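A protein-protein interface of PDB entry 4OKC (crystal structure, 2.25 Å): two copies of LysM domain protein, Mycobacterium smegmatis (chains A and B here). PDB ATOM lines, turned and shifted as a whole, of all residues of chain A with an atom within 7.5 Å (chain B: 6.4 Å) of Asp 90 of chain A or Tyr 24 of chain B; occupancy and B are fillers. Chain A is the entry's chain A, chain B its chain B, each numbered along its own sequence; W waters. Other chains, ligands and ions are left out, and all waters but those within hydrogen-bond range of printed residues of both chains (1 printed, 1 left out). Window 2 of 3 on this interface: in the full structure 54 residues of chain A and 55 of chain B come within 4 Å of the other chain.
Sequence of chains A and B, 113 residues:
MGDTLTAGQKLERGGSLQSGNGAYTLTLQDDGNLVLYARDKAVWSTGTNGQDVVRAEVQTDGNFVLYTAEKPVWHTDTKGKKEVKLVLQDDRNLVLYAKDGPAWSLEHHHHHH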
ATOM      1  N   VAL A  87      -1.556  -2.162 -15.986  1.00  0.00           N
ATOM      2  CA  VAL A  87      -1.176  -0.809 -16.346  1.00  0.00           C
ATOM      3  C   VAL A  87      -1.733  -0.451 -17.700  1.00  0.00           C
ATOM      4  O   VAL A  87      -1.515  -1.148 -18.687  1.00  0.00           O
ATOM      5  CB  VAL A  87       0.340  -0.619 -16.327  1.00  0.00           C
ATOM      6  CG1 VAL A  87       0.699   0.847 -16.620  1.00  0.00           C
ATOM      7  CG2 VAL A  87       0.930  -1.044 -14.998  1.00  0.00           C
ATOM      8  N   LEU A  88      -2.493   0.630 -17.737  1.00  0.00           N
ATOM      9  CA  LEU A  88      -2.986   1.160 -18.974  1.00  0.00           C
ATOM     10  C   LEU A  88      -1.880   2.093 -19.482  1.00  0.00           C
ATOM     11  O   LEU A  88      -1.521   3.058 -18.816  1.00  0.00           O
ATOM     12  CB  LEU A  88      -4.290   1.942 -18.726  1.00  0.00           C
ATOM     13  CG  LEU A  88      -4.889   2.705 -19.925  1.00  0.00           C
ATOM     14  CD1 LEU A  88      -5.352   1.750 -20.953  1.00  0.00           C
ATOM     15  CD2 LEU A  88      -6.035   3.622 -19.533  1.00  0.00           C
ATOM     16  N   GLN A  89      -1.359   1.833 -20.683  1.00  0.00           N
ATOM     17  CA  GLN A  89      -0.161   2.510 -21.125  1.00  0.00           C
ATOM     18  C   GLN A  89      -0.505   3.603 -22.075  1.00  0.00           C
ATOM     19  O   GLN A  89      -1.574   3.602 -22.673  1.00  0.00           O
ATOM     20  CB  GLN A  89       0.781   1.518 -21.784  1.00  0.00           C
ATOM     21  CG  GLN A  89       1.210   0.431 -20.855  1.00  0.00           C
ATOM     22  CD  GLN A  89       2.251  -0.480 -21.485  1.00  0.00           C
ATOM     23  OE1 GLN A  89       2.176  -0.802 -22.654  1.00  0.00           O
ATOM     24  NE2 GLN A  89       3.185  -0.953 -20.677  1.00  0.00           N
ATOM     25  N   ASP A  90       0.441   4.532 -22.226  1.00  0.00           N
ATOM     26  CA  ASP A  90       0.317   5.671 -23.131  1.00  0.00           C
ATOM     27  C   ASP A  90       0.265   5.263 -24.566  1.00  0.00           C
ATOM     28  O   ASP A  90      -0.244   6.039 -25.382  1.00  0.00           O
ATOM     29  CB  ASP A  90       1.444   6.661 -22.896  1.00  0.00           C
ATOM     30  CG  ASP A  90       1.277   7.394 -21.625  1.00  0.00           C
ATOM     31  OD1 ASP A  90       0.112   7.501 -21.148  1.00  0.00           O
ATOM     32  OD2 ASP A  90       2.308   7.822 -21.074  1.00  0.00           O
ATOM     33  N   ASP A  91       0.754   4.042 -24.861  1.00  0.00           N
ATOM     34  CA  ASP A  91       0.690   3.450 -26.221  1.00  0.00           C
ATOM     35  C   ASP A  91      -0.662   2.782 -26.484  1.00  0.00           C
ATOM     36  O   ASP A  91      -0.900   2.202 -27.545  1.00  0.00           O
ATOM     37  CB  ASP A  91       1.898   2.508 -26.510  1.00  0.00           C
ATOM     38  CG  ASP A  91       1.927   1.283 -25.627  1.00  0.00           C
ATOM     39  OD1 ASP A  91       1.035   1.122 -24.781  1.00  0.00           O
ATOM     40  OD2 ASP A  91       2.839   0.441 -25.782  1.00  0.00           O
ATOM     41  N   ARG A  92      -1.559   2.924 -25.503  1.00  0.00           N
ATOM     42  CA  ARG A  92      -2.948   2.384 -25.516  1.00  0.00           C
ATOM     43  C   ARG A  92      -3.068   0.883 -25.188  1.00  0.00           C
ATOM     44  O   ARG A  92      -4.127   0.281 -25.366  1.00  0.00           O
ATOM     45  CB  ARG A  92      -3.676   2.678 -26.822  1.00  0.00           C
ATOM     46  CG  ARG A  92      -5.214   2.551 -26.623  1.00  0.00           C
ATOM     47  CD  ARG A  92      -5.964   2.804 -27.884  1.00  0.00           C
ATOM     48  NE  ARG A  92      -5.974   1.610 -28.704  1.00  0.00           N
ATOM     49  CZ  ARG A  92      -6.372   1.553 -29.972  1.00  0.00           C
ATOM     50  NH1 ARG A  92      -6.802   2.641 -30.587  1.00  0.00           N
ATOM     51  NH2 ARG A  92      -6.357   0.376 -30.602  1.00  0.00           N
ATOM     52  N   ASN A  93      -1.961   0.264 -24.800  1.00  0.00           N
ATOM     53  CA  ASN A  93      -2.011  -1.116 -24.420  1.00  0.00           C
ATOM     54  C   ASN A  93      -2.260  -1.228 -22.897  1.00  0.00           C
ATOM     55  O   ASN A  93      -1.811  -0.393 -22.089  1.00  0.00           O
ATOM     56  CB  ASN A  93      -0.729  -1.837 -24.875  1.00  0.00           C
ATOM     57  CG  ASN A  93      -0.846  -3.358 -24.835  1.00  0.00           C
ATOM     58  OD1 ASN A  93      -1.938  -3.914 -24.691  1.00  0.00           O
ATOM     59  ND2 ASN A  93       0.313  -4.050 -24.924  1.00  0.00           N
ATOM     60  N   ASP B   3      -2.965   5.267 -13.156  1.00  0.00           N
ATOM     61  CA  ASP B   3      -2.777   4.428 -14.357  1.00  0.00           C
ATOM     62  C   ASP B   3      -2.476   2.962 -14.038  1.00  0.00           C
ATOM     63  O   ASP B   3      -2.288   2.166 -14.958  1.00  0.00           O
ATOM     64  CB  ASP B   3      -1.657   4.985 -15.226  1.00  0.00           C
ATOM     65  CG  ASP B   3      -0.276   4.855 -14.576  1.00  0.00           C
ATOM     66  OD1 ASP B   3      -0.106   4.189 -13.514  1.00  0.00           O
ATOM     67  OD2 ASP B   3       0.665   5.428 -15.156  1.00  0.00           O
ATOM     68  N   LEU B  17      -9.202   3.905 -14.660  1.00  0.00           N
ATOM     69  CA  LEU B  17      -7.765   4.141 -14.824  1.00  0.00           C
ATOM     70  C   LEU B  17      -7.627   4.986 -16.066  1.00  0.00           C
ATOM     71  O   LEU B  17      -8.453   4.873 -17.000  1.00  0.00           O
ATOM     72  CB  LEU B  17      -7.015   2.845 -15.059  1.00  0.00           C
ATOM     73  CG  LEU B  17      -6.670   1.888 -13.897  1.00  0.00           C
ATOM     74  CD1 LEU B  17      -5.676   0.741 -14.359  1.00  0.00           C
ATOM     75  CD2 LEU B  17      -6.147   2.608 -12.625  1.00  0.00           C
ATOM     76  N   GLN B  18      -6.629   5.874 -16.030  1.00  0.00           N
ATOM     77  CA  GLN B  18      -6.376   6.811 -17.092  1.00  0.00           C
ATOM     78  C   GLN B  18      -4.915   6.728 -17.444  1.00  0.00           C
ATOM     79  O   GLN B  18      -4.082   6.354 -16.595  1.00  0.00           O
ATOM     80  CB  GLN B  18      -6.774   8.223 -16.673  1.00  0.00           C
ATOM     81  CG  GLN B  18      -7.145   9.132 -17.843  1.00  0.00           C
ATOM     82  CD  GLN B  18      -7.708  10.431 -17.382  1.00  0.00           C
ATOM     83  OE1 GLN B  18      -6.960  11.381 -17.097  1.00  0.00           O
ATOM     84  NE2 GLN B  18      -9.036  10.513 -17.300  1.00  0.00           N
ATOM     85  N   SER B  19      -4.613   7.016 -18.711  1.00  0.00           N
ATOM     86  CA  SER B  19      -3.239   7.025 -19.237  1.00  0.00           C
ATOM     87  C   SER B  19      -2.475   8.247 -18.761  1.00  0.00           C
ATOM     88  O   SER B  19      -3.069   9.302 -18.498  1.00  0.00           O
ATOM     89  CB  SER B  19      -3.258   7.061 -20.773  1.00  0.00           C
ATOM     90  OG  SER B  19      -3.751   5.838 -21.254  1.00  0.00           O
ATOM     91  N   GLY B  20      -1.152   8.110 -18.720  1.00  0.00           N
ATOM     92  CA  GLY B  20      -0.266   9.210 -18.327  1.00  0.00           C
ATOM     93  C   GLY B  20      -0.566  10.473 -19.099  1.00  0.00           C
ATOM     94  O   GLY B  20      -0.864  11.525 -18.504  1.00  0.00           O
ATOM     95  N   ASN B  21      -0.434  10.385 -20.424  1.00  0.00           N
ATOM     96  CA  ASN B  21      -0.713  11.506 -21.332  1.00  0.00           C
ATOM     97  C   ASN B  21      -2.205  11.835 -21.295  1.00  0.00           C
ATOM     98  O   ASN B  21      -2.656  12.821 -21.884  1.00  0.00           O
ATOM     99  CB  ASN B  21      -0.242  11.166 -22.759  1.00  0.00           C
ATOM    100  CG  ASN B  21      -0.785   9.805 -23.279  1.00  0.00           C
ATOM    101  OD1 ASN B  21      -0.245   9.216 -24.241  1.00  0.00           O
ATOM    102  ND2 ASN B  21      -1.882   9.324 -22.663  1.00  0.00           N
ATOM    103  N   GLY B  22      -2.972  10.994 -20.594  1.00  0.00           N
ATOM    104  CA  GLY B  22      -4.415  11.213 -20.387  1.00  0.00           C
ATOM    105  C   GLY B  22      -5.302  10.856 -21.568  1.00  0.00           C
ATOM    106  O   GLY B  22      -6.504  10.955 -21.490  1.00  0.00           O
ATOM    107  N   ALA B  23      -4.680  10.421 -22.651  1.00  0.00           N
ATOM    108  CA  ALA B  23      -5.381  10.043 -23.885  1.00  0.00           C
ATOM    109  C   ALA B  23      -6.379   8.876 -23.727  1.00  0.00           C
ATOM    110  O   ALA B  23      -7.413   8.852 -24.431  1.00  0.00           O
ATOM    111  CB  ALA B  23      -4.368   9.688 -24.915  1.00  0.00           C
ATOM    112  N   TYR B  24      -6.077   7.910 -22.842  1.00  0.00           N
ATOM    113  CA  TYR B  24      -6.843   6.678 -22.770  1.00  0.00           C
ATOM    114  C   TYR B  24      -7.379   6.403 -21.379  1.00  0.00           C
ATOM    115  O   TYR B  24      -6.761   6.731 -20.375  1.00  0.00           O
ATOM    116  CB  TYR B  24      -6.031   5.471 -23.272  1.00  0.00           C
ATOM    117  CG  TYR B  24      -5.183   5.778 -24.491  1.00  0.00           C
ATOM    118  CD1 TYR B  24      -5.777   6.145 -25.719  1.00  0.00           C
ATOM    119  CD2 TYR B  24      -3.810   5.730 -24.419  1.00  0.00           C
ATOM    120  CE1 TYR B  24      -5.006   6.443 -26.837  1.00  0.00           C
ATOM    121  CE2 TYR B  24      -3.034   6.013 -25.542  1.00  0.00           C
ATOM    122  CZ  TYR B  24      -3.630   6.376 -26.728  1.00  0.00           C
ATOM    123  OH  TYR B  24      -2.836   6.661 -27.810  1.00  0.00           O
ATOM    124  N   THR B  25      -8.573   5.846 -21.337  1.00  0.00           N
ATOM    125  CA  THR B  25      -9.262   5.614 -20.081  1.00  0.00           C
ATOM    126  C   THR B  25      -9.798   4.170 -20.075  1.00  0.00           C
ATOM    127  O   THR B  25     -10.147   3.619 -21.104  1.00  0.00           O
ATOM    128  CB  THR B  25     -10.469   6.551 -19.926  1.00  0.00           C
ATOM    129  OG1 THR B  25     -10.016   7.908 -19.978  1.00  0.00           O
ATOM    130  CG2 THR B  25     -11.186   6.295 -18.595  1.00  0.00           C
ATOM    131  N   LEU B  26      -9.873   3.579 -18.905  1.00  0.00           N
ATOM    132  CA  LEU B  26     -10.445   2.285 -18.755  1.00  0.00           C
ATOM    133  C   LEU B  26     -11.357   2.411 -17.548  1.00  0.00           C
ATOM    134  O   LEU B  26     -10.875   2.515 -16.419  1.00  0.00           O
ATOM    135  CB  LEU B  26      -9.349   1.278 -18.451  1.00  0.00           C
ATOM    136  CG  LEU B  26      -9.865  -0.127 -18.211  1.00  0.00           C
ATOM    137  CD1 LEU B  26     -10.424  -0.674 -19.540  1.00  0.00           C
ATOM    138  CD2 LEU B  26      -8.773  -1.060 -17.556  1.00  0.00           C
ATOM    139  N   LEU B  36     -12.396   0.262 -22.585  1.00  0.00           N
ATOM    140  CA  LEU B  36     -11.225   1.092 -22.806  1.00  0.00           C
ATOM    141  C   LEU B  36     -11.507   2.201 -23.840  1.00  0.00           C
ATOM    142  O   LEU B  36     -11.759   1.956 -25.036  1.00  0.00           O
ATOM    143  CB  LEU B  36     -10.060   0.218 -23.269  1.00  0.00           C
ATOM    144  CG  LEU B  36      -8.761   0.942 -23.699  1.00  0.00           C
ATOM    145  CD1 LEU B  36      -8.337   2.182 -22.833  1.00  0.00           C
ATOM    146  CD2 LEU B  36      -7.605  -0.010 -23.862  1.00  0.00           C
ATOM    147  N   TYR B  37     -11.448   3.443 -23.384  1.00  0.00           N
ATOM    148  CA  TYR B  37     -11.695   4.550 -24.272  1.00  0.00           C
ATOM    149  C   TYR B  37     -10.426   5.254 -24.725  1.00  0.00           C
ATOM    150  O   TYR B  37      -9.504   5.400 -23.927  1.00  0.00           O
ATOM    151  CB  TYR B  37     -12.582   5.561 -23.604  1.00  0.00           C
ATOM    152  CG  TYR B  37     -13.992   5.062 -23.396  1.00  0.00           C
ATOM    153  CD1 TYR B  37     -14.867   4.886 -24.463  1.00  0.00           C
ATOM    154  CD2 TYR B  37     -14.441   4.767 -22.113  1.00  0.00           C
ATOM    155  CE1 TYR B  37     -16.206   4.431 -24.222  1.00  0.00           C
ATOM    156  CE2 TYR B  37     -15.710   4.340 -21.881  1.00  0.00           C
ATOM    157  CZ  TYR B  37     -16.581   4.173 -22.905  1.00  0.00           C
ATOM    158  OH  TYR B  37     -17.826   3.743 -22.591  1.00  0.00           O
ATOM    159  N   ALA B  38     -10.417   5.653 -26.013  1.00  0.00           N
ATOM    160  CA  ALA B  38      -9.443   6.559 -26.596  1.00  0.00           C
ATOM    161  C   ALA B  38     -10.246   7.785 -27.005  1.00  0.00           C
ATOM    162  O   ALA B  38     -10.923   7.787 -28.053  1.00  0.00           O
ATOM    163  CB  ALA B  38      -8.788   5.942 -27.786  1.00  0.00           C
ATOM    164  N   ARG B  39     -10.191   8.817 -26.170  1.00  0.00           N
ATOM    165  CA  ARG B  39     -11.044   9.988 -26.356  1.00  0.00           C
ATOM    166  C   ARG B  39     -12.528   9.546 -26.521  1.00  0.00           C
ATOM    167  O   ARG B  39     -13.072   8.872 -25.654  1.00  0.00           O
ATOM    168  CB  ARG B  39     -10.577  10.828 -27.567  1.00  0.00           C
ATOM    169  CG  ARG B  39      -9.151  11.209 -27.519  1.00  0.00           C
ATOM    170  CD  ARG B  39      -8.640  11.825 -28.821  1.00  0.00           C
ATOM    171  NE  ARG B  39      -7.284  12.303 -28.564  1.00  0.00           N
ATOM    172  CZ  ARG B  39      -6.246  11.486 -28.384  1.00  0.00           C
ATOM    173  NH1 ARG B  39      -6.407  10.167 -28.477  1.00  0.00           N
ATOM    174  NH2 ARG B  39      -5.049  11.981 -28.114  1.00  0.00           N
HETATM  175  O   HOH W   1      -2.538   3.978 -29.612  1.00  0.00           O
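The side-chain carboxylate (OD1) of Asp 90 of chain A sits at hydrogen-bond distance from the backbone NH (N) of Asn 21 of chain B, at 3.0 Å.
O of Gln 89 of chain A sits at hydrogen-bond distance from OG of Ser 19 of chain B, at 3.4 Å.
O of Asp 3 of chain B sits at hydrogen-bond distance from N of Leu 88 of chain A, 3.2 Å away.
The side-chain carboxylate of Asp 90 of chain A is in hydrogen-bond range of the backbone NH of Gly 20 of chain B.
O of Leu 17 of chain B lies within hydrogen-bond range of N of Leu 26 of chain B (2.7 Å).
The side-chain amide nitrogen (ND2) of Asn 21 of chain B lies close to the backbone NH (N) of Ala 23 of chain B (3.0 Å).
N of Ser 19 of chain B sits at hydrogen-bond distance from O of Tyr 24 of chain B.
The side-chain carboxylate (OD1) of Asp 91 of chain A lies close to the side-chain amide oxygen (OE1) of Gln 89 of chain A.
The backbone NH (N) of Tyr 37 of chain B is in hydrogen-bond range of the backbone carbonyl oxygen (O) of Thr 25 of chain B (2.6 Å).
Among the printed residues, pairs that only touch across the chains: Asp 90 of chain A with Tyr 24 of chain B (2.8 Å), Leu 88 of chain A with Tyr 24 of chain B (3.3 Å), Asp 90 of chain A with Ser 19 of chain B (3.4 Å), Arg 92 of chain A with Tyr 24 of chain B (3.4 Å), Val 87 of chain A with Asp 3 of chain B (3.5 Å), Gln 89 of chain A with Tyr 24 of chain B (3.5 Å), Leu 88 of chain A with Leu 36 of chain B (3.6 Å), Leu 88 of chain A with Ser 19 of chain B (3.6 Å), Leu 88 of chain A with Leu 17 of chain B (3.7 Å), Arg 92 of chain A with Leu 36 of chain B (3.8 Å), Leu 88 of chain A with Thr 25 of chain B (3.8 Å), Leu 88 of chain A with Leu 26 of chain B (3.9 Å) and Leu 88 of chain A with Gln 18 of chain B (3.9 Å).
Asp 90 of chain A touches four residues of chain B.
Tyr 24 of chain B touches four residues of chain A.
Of the printed residues of chain B, Arg 92 of chain A touches Tyr 24 and Leu 36.
Printed residues of chain A within 4 Å of Gln 18 of chain B: Leu 88.
Of the printed residues of chain A, Gly 20 of chain B touches Asp 90.
Of the printed residues of chain B, Gln 89 of chain A touches Ser 19 (3.4 Å) and Tyr 24 (3.5 Å).
Ala 38 of chain B touches none of the printed residues of chain A.
The nearest residue of chain A that does not touch Tyr 24 of chain B is Asp 91 of chain A (4.1 Å).
The nearest printed residue of chain A that does not touch Asn 21 of chain B is Asp 91 of chain A (5.3 Å).
Hydrophobic or aromatic side chains of chain B within 4 Å of the printed part of chain A: Tyr 24 and Leu 36.
Printed residues of chain A that touch a printed residue of chain B: Val 87, Leu 88, Gln 89, Asp 90 and Arg 92.
Hydrophobic or aromatic side chains of chain A that line the printed part of chain B: Val 87 and Leu 88.
Among the printed residues, no Asp or Glu carboxylate lies within 4 Å of a Lys or Arg side-chain nitrogen of the other chain.
No position is printed for both chains.
Water W1 lies within hydrogen-bond range of O of Asp 91 of chain A (3.2 Å) and OH of Tyr 24 of chain B (3.2 Å).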
